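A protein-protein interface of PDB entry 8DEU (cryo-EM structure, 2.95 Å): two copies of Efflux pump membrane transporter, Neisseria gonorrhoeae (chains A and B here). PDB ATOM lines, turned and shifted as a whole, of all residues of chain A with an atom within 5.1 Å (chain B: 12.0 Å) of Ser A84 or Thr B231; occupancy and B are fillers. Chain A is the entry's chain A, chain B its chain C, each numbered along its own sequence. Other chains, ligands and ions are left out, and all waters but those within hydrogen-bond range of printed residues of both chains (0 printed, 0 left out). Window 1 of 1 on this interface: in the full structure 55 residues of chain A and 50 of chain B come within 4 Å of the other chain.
No position is printed for both chains.
The backbone carbonyl oxygen (O) of Thr B231 sits at hydrogen-bond distance from the backbone NH (N) of Leu A724. The backbone carbonyl oxygen (O) of Leu A724 is in hydrogen-bond range of the backbone NH (N) of Thr B233 (3.0 Å).
Among the printed residues, merely in contact across the chains: Ser A84 with Thr B231 (3.5 Å), Pro A722 with Ala B230 (3.97 Å), Gln A723 with Thr B231 (3.3 Å), Leu A724 with Ile B217 (3.2 Å), Leu A724 with Val B232 (3.5 Å) and Glu A811 with Thr B231 (3.6 Å).
Ser A84 touches just one residue of chain B: Thr B231. Thr B231 touches just these residues of chain A: Ser A84, Gln A723, Leu A724 and Glu A811. No residue of chain B comes within 4 Å of Ala A52. No residue of chain B comes within 4 Å of Ser A53. No residue of chain B comes within 4 Å of Ala A54. No residue of chain B comes within 4 Å of Ala A82. No residue of chain B comes within 4 Å of Asp A83. No residue of chain B comes within 4 Å of Gly A86. Of chain B, only Ile B217, Thr B231, Val B232 and Thr B233 come within 4 Å of Leu A724. Glu A811 touches one residue of chain B. Printed residues of chain A within 4 Å of Thr B233: Leu A724 (3.0 Å). Printed residues of chain B within 4 Å of Pro A722: Ala B230 (3.97 Å). Ala B234 touches none of the printed residues of chain A. The nearest printed residue of chain A that does not touch Val B232 is Ser A53 (5.2 Å).
The side-chain carboxylate of Glu A811 is in hydrogen-bond range of the side-chain hydroxyl of Ser A84 (2.9 Å). The side-chain amide nitrogen (NE2) of Gln A723 sits at hydrogen-bond distance from the side-chain carboxylate (OE2) of Glu A811. O of Gly B215 sits at hydrogen-bond distance from N of Val B232 (3.1 Å). The backbone NH (N) of Ile B217 lies within hydrogen-bond range of the backbone carbonyl oxygen (O) of Ala B230 (2.7 Å).
Of the 12 printed residues of chain A, 5 touch a printed residue of chain B. Hydrophobic or aromatic side chains of chain A that line the printed part of chain B: Leu A724. Along chain A the printed residues that touch a printed residue of chain B span positions 84 to 811. Of the 20 printed residues of chain B, 5 touch a printed residue of chain A. Printed residues of chain B that touch a printed residue of chain A: Ile B217, Ala B230, Thr B231, Val B232 and Thr B233. Hydrophobic or aromatic side chains of chain B within 4 Å of the printed part of chain A: Ile B217 and Ala B230.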
ATOM      1  N   ALA A  52      -9.674  -4.336  -1.944  1.00  0.00           N
ATOM      2  CA  ALA A  52     -10.753  -3.390  -2.184  1.00  0.00           C
ATOM      3  C   ALA A  52     -10.697  -2.806  -3.576  1.00  0.00           C
ATOM      4  O   ALA A  52      -9.631  -2.416  -4.041  1.00  0.00           O
ATOM      5  CB  ALA A  52     -10.704  -2.280  -1.160  1.00  0.00           C
ATOM      6  N   SER A  53     -11.845  -2.700  -4.247  1.00  0.00           N
ATOM      7  CA  SER A  53     -11.893  -2.130  -5.585  1.00  0.00           C
ATOM      8  C   SER A  53     -11.588  -0.647  -5.566  1.00  0.00           C
ATOM      9  O   SER A  53     -11.428  -0.062  -4.513  1.00  0.00           O
ATOM     10  CB  SER A  53     -13.272  -2.354  -6.193  1.00  0.00           C
ATOM     11  OG  SER A  53     -14.264  -1.649  -5.474  1.00  0.00           O
ATOM     12  N   ALA A  54     -11.487  -0.030  -6.733  1.00  0.00           N
ATOM     13  CA  ALA A  54     -11.273   1.403  -6.790  1.00  0.00           C
ATOM     14  C   ALA A  54     -12.465   2.111  -6.190  1.00  0.00           C
ATOM     15  O   ALA A  54     -12.312   3.137  -5.551  1.00  0.00           O
ATOM     16  CB  ALA A  54     -11.058   1.843  -8.219  1.00  0.00           C
ATOM     17  N   ALA A  82      -7.389   6.277  -6.804  1.00  0.00           N
ATOM     18  CA  ALA A  82      -7.532   4.934  -6.273  1.00  0.00           C
ATOM     19  C   ALA A  82      -7.439   3.936  -7.406  1.00  0.00           C
ATOM     20  O   ALA A  82      -7.611   4.293  -8.564  1.00  0.00           O
ATOM     21  CB  ALA A  82      -8.859   4.793  -5.563  1.00  0.00           C
ATOM     22  N   ASP A  83      -7.170   2.682  -7.078  1.00  0.00           N
ATOM     23  CA  ASP A  83      -7.042   1.639  -8.091  1.00  0.00           C
ATOM     24  C   ASP A  83      -7.344   0.262  -7.509  1.00  0.00           C
ATOM     25  O   ASP A  83      -7.515   0.128  -6.298  1.00  0.00           O
ATOM     26  CB  ASP A  83      -5.684   1.684  -8.803  1.00  0.00           C
ATOM     27  CG  ASP A  83      -4.515   1.850  -7.851  1.00  0.00           C
ATOM     28  OD1 ASP A  83      -4.570   1.335  -6.720  1.00  0.00           O
ATOM     29  OD2 ASP A  83      -3.520   2.490  -8.250  1.00  0.00           O
ATOM     30  N   SER A  84      -7.430  -0.756  -8.356  1.00  0.00           N
ATOM     31  CA  SER A  84      -7.792  -2.098  -7.898  1.00  0.00           C
ATOM     32  C   SER A  84      -6.766  -2.824  -7.031  1.00  0.00           C
ATOM     33  O   SER A  84      -7.090  -3.833  -6.412  1.00  0.00           O
ATOM     34  CB  SER A  84      -8.216  -2.962  -9.078  1.00  0.00           C
ATOM     35  OG  SER A  84      -9.537  -2.634  -9.470  1.00  0.00           O
ATOM     36  N   SER A  85      -5.539  -2.327  -6.979  1.00  0.00           N
ATOM     37  CA  SER A  85      -4.484  -2.953  -6.188  1.00  0.00           C
ATOM     38  C   SER A  85      -4.777  -3.036  -4.702  1.00  0.00           C
ATOM     39  O   SER A  85      -4.376  -3.996  -4.054  1.00  0.00           O
ATOM     40  CB  SER A  85      -3.169  -2.204  -6.389  1.00  0.00           C
ATOM     41  OG  SER A  85      -3.181  -0.956  -5.727  1.00  0.00           O
ATOM     42  N   GLY A  86      -5.447  -2.041  -4.144  1.00  0.00           N
ATOM     43  CA  GLY A  86      -5.664  -2.001  -2.705  1.00  0.00           C
ATOM     44  C   GLY A  86      -4.925  -0.847  -2.053  1.00  0.00           C
ATOM     45  O   GLY A  86      -4.609  -0.920  -0.874  1.00  0.00           O
ATOM     46  N   PRO A 722     -13.502  -5.795 -17.765  1.00  0.00           N
ATOM     47  CA  PRO A 722     -14.606  -6.637 -17.296  1.00  0.00           C
ATOM     48  C   PRO A 722     -14.461  -6.978 -15.822  1.00  0.00           C
ATOM     49  O   PRO A 722     -13.355  -7.128 -15.298  1.00  0.00           O
ATOM     50  CB  PRO A 722     -14.493  -7.891 -18.169  1.00  0.00           C
ATOM     51  CG  PRO A 722     -13.661  -7.477 -19.332  1.00  0.00           C
ATOM     52  CD  PRO A 722     -12.706  -6.465 -18.802  1.00  0.00           C
ATOM     53  N   GLN A 723     -15.601  -7.099 -15.149  1.00  0.00           N
ATOM     54  CA  GLN A 723     -15.627  -7.390 -13.726  1.00  0.00           C
ATOM     55  C   GLN A 723     -16.769  -8.347 -13.425  1.00  0.00           C
ATOM     56  O   GLN A 723     -17.752  -8.423 -14.164  1.00  0.00           O
ATOM     57  CB  GLN A 723     -15.781  -6.116 -12.894  1.00  0.00           C
ATOM     58  CG  GLN A 723     -14.750  -5.058 -13.197  1.00  0.00           C
ATOM     59  CD  GLN A 723     -14.983  -3.794 -12.414  1.00  0.00           C
ATOM     60  OE1 GLN A 723     -16.102  -3.506 -12.002  1.00  0.00           O
ATOM     61  NE2 GLN A 723     -13.925  -3.027 -12.203  1.00  0.00           N
ATOM     62  N   LEU A 724     -16.628  -9.077 -12.325  1.00  0.00           N
ATOM     63  CA  LEU A 724     -17.658  -9.989 -11.853  1.00  0.00           C
ATOM     64  C   LEU A 724     -18.520  -9.278 -10.821  1.00  0.00           C
ATOM     65  O   LEU A 724     -17.997  -8.617  -9.919  1.00  0.00           O
ATOM     66  CB  LEU A 724     -17.040 -11.248 -11.252  1.00  0.00           C
ATOM     67  CG  LEU A 724     -16.757 -12.379 -12.236  1.00  0.00           C
ATOM     68  CD1 LEU A 724     -15.941 -13.461 -11.567  1.00  0.00           C
ATOM     69  CD2 LEU A 724     -18.055 -12.942 -12.767  1.00  0.00           C
ATOM     70  N   GLU A 811     -11.497   0.630 -13.624  1.00  0.00           N
ATOM     71  CA  GLU A 811     -10.402   0.128 -12.809  1.00  0.00           C
ATOM     72  C   GLU A 811      -9.689   1.219 -12.027  1.00  0.00           C
ATOM     73  O   GLU A 811      -8.882   0.902 -11.151  1.00  0.00           O
ATOM     74  CB  GLU A 811      -9.383  -0.608 -13.684  1.00  0.00           C
ATOM     75  CG  GLU A 811      -9.885  -1.925 -14.242  1.00  0.00           C
ATOM     76  CD  GLU A 811     -10.081  -2.974 -13.170  1.00  0.00           C
ATOM     77  OE1 GLU A 811      -9.170  -3.146 -12.335  1.00  0.00           O
ATOM     78  OE2 GLU A 811     -11.145  -3.626 -13.162  1.00  0.00           O
ATOM     79  N   ILE B 212     -18.637  -4.743   1.381  1.00  0.00           N
ATOM     80  CA  ILE B 212     -17.975  -6.026   1.183  1.00  0.00           C
ATOM     81  C   ILE B 212     -16.854  -5.884   0.174  1.00  0.00           C
ATOM     82  O   ILE B 212     -17.087  -5.416  -0.935  1.00  0.00           O
ATOM     83  CB  ILE B 212     -18.959  -7.076   0.642  1.00  0.00           C
ATOM     84  CG1 ILE B 212     -20.231  -7.116   1.490  1.00  0.00           C
ATOM     85  CG2 ILE B 212     -18.301  -8.445   0.579  1.00  0.00           C
ATOM     86  CD1 ILE B 212     -21.279  -8.068   0.959  1.00  0.00           C
ATOM     87  N   SER B 213     -15.637  -6.284   0.534  1.00  0.00           N
ATOM     88  CA  SER B 213     -14.545  -6.268  -0.434  1.00  0.00           C
ATOM     89  C   SER B 213     -14.206  -7.691  -0.853  1.00  0.00           C
ATOM     90  O   SER B 213     -13.485  -8.393  -0.153  1.00  0.00           O
ATOM     91  CB  SER B 213     -13.331  -5.551   0.150  1.00  0.00           C
ATOM     92  OG  SER B 213     -13.090  -5.941   1.488  1.00  0.00           O
ATOM     93  N   ALA B 214     -14.721  -8.118  -1.999  1.00  0.00           N
ATOM     94  CA  ALA B 214     -14.497  -9.483  -2.468  1.00  0.00           C
ATOM     95  C   ALA B 214     -13.082  -9.843  -2.887  1.00  0.00           C
ATOM     96  O   ALA B 214     -12.601 -10.927  -2.571  1.00  0.00           O
ATOM     97  CB  ALA B 214     -15.478  -9.809  -3.576  1.00  0.00           C
ATOM     98  N   GLY B 215     -12.409  -9.021  -3.690  1.00  0.00           N
ATOM     99  CA  GLY B 215     -11.086  -9.396  -4.177  1.00  0.00           C
ATOM    100  C   GLY B 215     -10.959  -9.528  -5.685  1.00  0.00           C
ATOM    101  O   GLY B 215     -11.605  -8.785  -6.407  1.00  0.00           O
ATOM    102  N   SER B 216     -10.111 -10.439  -6.168  1.00  0.00           N
ATOM    103  CA  SER B 216      -9.895 -10.603  -7.614  1.00  0.00           C
ATOM    104  C   SER B 216      -9.708 -12.028  -8.127  1.00  0.00           C
ATOM    105  O   SER B 216      -9.183 -12.877  -7.416  1.00  0.00           O
ATOM    106  CB  SER B 216      -8.711  -9.758  -8.082  1.00  0.00           C
ATOM    107  OG  SER B 216      -8.985  -8.375  -7.981  1.00  0.00           O
ATOM    108  N   ILE B 217     -10.135 -12.292  -9.359  1.00  0.00           N
ATOM    109  CA  ILE B 217      -9.992 -13.612  -9.977  1.00  0.00           C
ATOM    110  C   ILE B 217      -8.562 -14.049 -10.236  1.00  0.00           C
ATOM    111  O   ILE B 217      -8.246 -15.208 -10.075  1.00  0.00           O
ATOM    112  CB  ILE B 217     -10.810 -13.711 -11.275  1.00  0.00           C
ATOM    113  CG1 ILE B 217     -12.172 -14.337 -11.003  1.00  0.00           C
ATOM    114  CG2 ILE B 217     -10.080 -14.515 -12.338  1.00  0.00           C
ATOM    115  CD1 ILE B 217     -12.979 -14.527 -12.266  1.00  0.00           C
ATOM    116  N   GLY B 218      -7.692 -13.163 -10.686  1.00  0.00           N
ATOM    117  CA  GLY B 218      -6.302 -13.545 -10.831  1.00  0.00           C
ATOM    118  C   GLY B 218      -5.555 -12.661  -9.870  1.00  0.00           C
ATOM    119  O   GLY B 218      -5.619 -11.441  -9.989  1.00  0.00           O
ATOM    120  N   SER B 219      -4.845 -13.243  -8.918  1.00  0.00           N
ATOM    121  CA  SER B 219      -4.187 -12.427  -7.914  1.00  0.00           C
ATOM    122  C   SER B 219      -2.693 -12.527  -8.081  1.00  0.00           C
ATOM    123  O   SER B 219      -2.223 -13.356  -8.851  1.00  0.00           O
ATOM    124  CB  SER B 219      -4.643 -12.795  -6.511  1.00  0.00           C
ATOM    125  OG  SER B 219      -6.050 -12.686  -6.392  1.00  0.00           O
ATOM    126  N   LEU B 220      -1.932 -11.707  -7.369  1.00  0.00           N
ATOM    127  CA  LEU B 220      -0.491 -11.660  -7.599  1.00  0.00           C
ATOM    128  C   LEU B 220       0.313 -12.927  -7.417  1.00  0.00           C
ATOM    129  O   LEU B 220       1.206 -13.194  -8.219  1.00  0.00           O
ATOM    130  CB  LEU B 220       0.140 -10.505  -6.831  1.00  0.00           C
ATOM    131  CG  LEU B 220       0.195  -9.197  -7.621  1.00  0.00           C
ATOM    132  CD1 LEU B 220       0.779  -9.469  -8.999  1.00  0.00           C
ATOM    133  CD2 LEU B 220      -1.185  -8.572  -7.738  1.00  0.00           C
ATOM    134  N   PRO B 221       0.034 -13.715  -6.370  1.00  0.00           N
ATOM    135  CA  PRO B 221       0.776 -14.980  -6.346  1.00  0.00           C
ATOM    136  C   PRO B 221      -0.080 -15.860  -7.232  1.00  0.00           C
ATOM    137  O   PRO B 221      -1.093 -16.370  -6.767  1.00  0.00           O
ATOM    138  CB  PRO B 221       0.720 -15.409  -4.883  1.00  0.00           C
ATOM    139  CG  PRO B 221       0.177 -14.240  -4.125  1.00  0.00           C
ATOM    140  CD  PRO B 221      -0.641 -13.444  -5.094  1.00  0.00           C
ATOM    141  N   GLN B 226      -1.752 -18.283 -16.249  1.00  0.00           N
ATOM    142  CA  GLN B 226      -2.903 -17.408 -16.095  1.00  0.00           C
ATOM    143  C   GLN B 226      -2.869 -16.291 -17.128  1.00  0.00           C
ATOM    144  O   GLN B 226      -1.817 -15.706 -17.397  1.00  0.00           O
ATOM    145  CB  GLN B 226      -2.934 -16.822 -14.685  1.00  0.00           C
ATOM    146  CG  GLN B 226      -4.121 -15.932 -14.409  1.00  0.00           C
ATOM    147  CD  GLN B 226      -5.408 -16.709 -14.292  1.00  0.00           C
ATOM    148  OE1 GLN B 226      -5.428 -17.923 -14.471  1.00  0.00           O
ATOM    149  NE2 GLN B 226      -6.495 -16.012 -13.992  1.00  0.00           N
ATOM    150  N   THR B 227      -4.031 -15.994 -17.707  1.00  0.00           N
ATOM    151  CA  THR B 227      -4.136 -15.012 -18.776  1.00  0.00           C
ATOM    152  C   THR B 227      -5.004 -13.809 -18.442  1.00  0.00           C
ATOM    153  O   THR B 227      -4.749 -12.727 -18.975  1.00  0.00           O
ATOM    154  CB  THR B 227      -4.684 -15.671 -20.051  1.00  0.00           C
ATOM    155  OG1 THR B 227      -3.741 -16.634 -20.535  1.00  0.00           O
ATOM    156  CG2 THR B 227      -4.917 -14.633 -21.126  1.00  0.00           C
ATOM    157  N   VAL B 228      -6.010 -13.953 -17.583  1.00  0.00           N
ATOM    158  CA  VAL B 228      -6.931 -12.865 -17.283  1.00  0.00           C
ATOM    159  C   VAL B 228      -7.086 -12.715 -15.778  1.00  0.00           C
ATOM    160  O   VAL B 228      -6.938 -13.676 -15.017  1.00  0.00           O
ATOM    161  CB  VAL B 228      -8.309 -13.081 -17.939  1.00  0.00           C
ATOM    162  CG1 VAL B 228      -8.239 -12.782 -19.424  1.00  0.00           C
ATOM    163  CG2 VAL B 228      -8.787 -14.498 -17.695  1.00  0.00           C
ATOM    164  N   THR B 229      -7.389 -11.490 -15.354  1.00  0.00           N
ATOM    165  CA  THR B 229      -7.672 -11.171 -13.961  1.00  0.00           C
ATOM    166  C   THR B 229      -8.857 -10.224 -13.919  1.00  0.00           C
ATOM    167  O   THR B 229      -8.843  -9.187 -14.586  1.00  0.00           O
ATOM    168  CB  THR B 229      -6.469 -10.523 -13.273  1.00  0.00           C
ATOM    169  OG1 THR B 229      -6.486  -9.112 -13.513  1.00  0.00           O
ATOM    170  CG2 THR B 229      -5.182 -11.090 -13.816  1.00  0.00           C
ATOM    171  N   ALA B 230      -9.876 -10.572 -13.140  1.00  0.00           N
ATOM    172  CA  ALA B 230     -11.091  -9.780 -13.049  1.00  0.00           C
ATOM    173  C   ALA B 230     -11.329  -9.371 -11.607  1.00  0.00           C
ATOM    174  O   ALA B 230     -10.971 -10.099 -10.680  1.00  0.00           O
ATOM    175  CB  ALA B 230     -12.299 -10.551 -13.577  1.00  0.00           C
ATOM    176  N   THR B 231     -11.929  -8.201 -11.424  1.00  0.00           N
ATOM    177  CA  THR B 231     -12.276  -7.706 -10.101  1.00  0.00           C
ATOM    178  C   THR B 231     -13.686  -8.142  -9.738  1.00  0.00           C
ATOM    179  O   THR B 231     -14.574  -8.181 -10.591  1.00  0.00           O
ATOM    180  CB  THR B 231     -12.171  -6.184 -10.054  1.00  0.00           C
ATOM    181  OG1 THR B 231     -10.823  -5.793 -10.322  1.00  0.00           O
ATOM    182  CG2 THR B 231     -12.567  -5.670  -8.692  1.00  0.00           C
ATOM    183  N   VAL B 232     -13.890  -8.467  -8.464  1.00  0.00           N
ATOM    184  CA  VAL B 232     -15.171  -8.946  -7.962  1.00  0.00           C
ATOM    185  C   VAL B 232     -15.774  -7.885  -7.054  1.00  0.00           C
ATOM    186  O   VAL B 232     -15.064  -7.255  -6.264  1.00  0.00           O
ATOM    187  CB  VAL B 232     -15.017 -10.286  -7.222  1.00  0.00           C
ATOM    188  CG1 VAL B 232     -16.369 -10.906  -6.973  1.00  0.00           C
ATOM    189  CG2 VAL B 232     -14.143 -11.225  -8.021  1.00  0.00           C
ATOM    190  N   THR B 233     -17.088  -7.686  -7.171  1.00  0.00           N
ATOM    191  CA  THR B 233     -17.806  -6.671  -6.413  1.00  0.00           C
ATOM    192  C   THR B 233     -19.071  -7.272  -5.823  1.00  0.00           C
ATOM    193  O   THR B 233     -19.684  -8.162  -6.414  1.00  0.00           O
ATOM    194  CB  THR B 233     -18.169  -5.469  -7.289  1.00  0.00           C
ATOM    195  OG1 THR B 233     -19.265  -5.817  -8.140  1.00  0.00           O
ATOM    196  CG2 THR B 233     -16.987  -5.060  -8.147  1.00  0.00           C
ATOM    197  N   ALA B 234     -19.466  -6.773  -4.651  1.00  0.00           N
ATOM    198  CA  ALA B 234     -20.593  -7.334  -3.917  1.00  0.00           C
ATOM    199  C   ALA B 234     -21.726  -6.345  -3.693  1.00  0.00           C
ATOM    200  O   ALA B 234     -22.885  -6.670  -3.971  1.00  0.00           O
ATOM    201  CB  ALA B 234     -20.113  -7.888  -2.569  1.00  0.00           C
ATOM    202  N   GLN B 235     -21.434  -5.138  -3.208  1.00  0.00           N
ATOM    203  CA  GLN B 235     -22.462  -4.137  -2.911  1.00  0.00           C
ATOM    204  C   GLN B 235     -23.440  -4.637  -1.841  1.00  0.00           C
ATOM    205  O   GLN B 235     -24.606  -4.934  -2.101  1.00  0.00           O
ATOM    206  CB  GLN B 235     -23.214  -3.727  -4.181  1.00  0.00           C
ATOM    207  CG  GLN B 235     -24.353  -2.760  -3.919  1.00  0.00           C
ATOM    208  CD  GLN B 235     -23.944  -1.609  -3.028  1.00  0.00           C
ATOM    209  OE1 GLN B 235     -24.674  -1.224  -2.121  1.00  0.00           O
ATOM    210  NE2 GLN B 235     -22.774  -1.046  -3.287  1.00  0.00           N
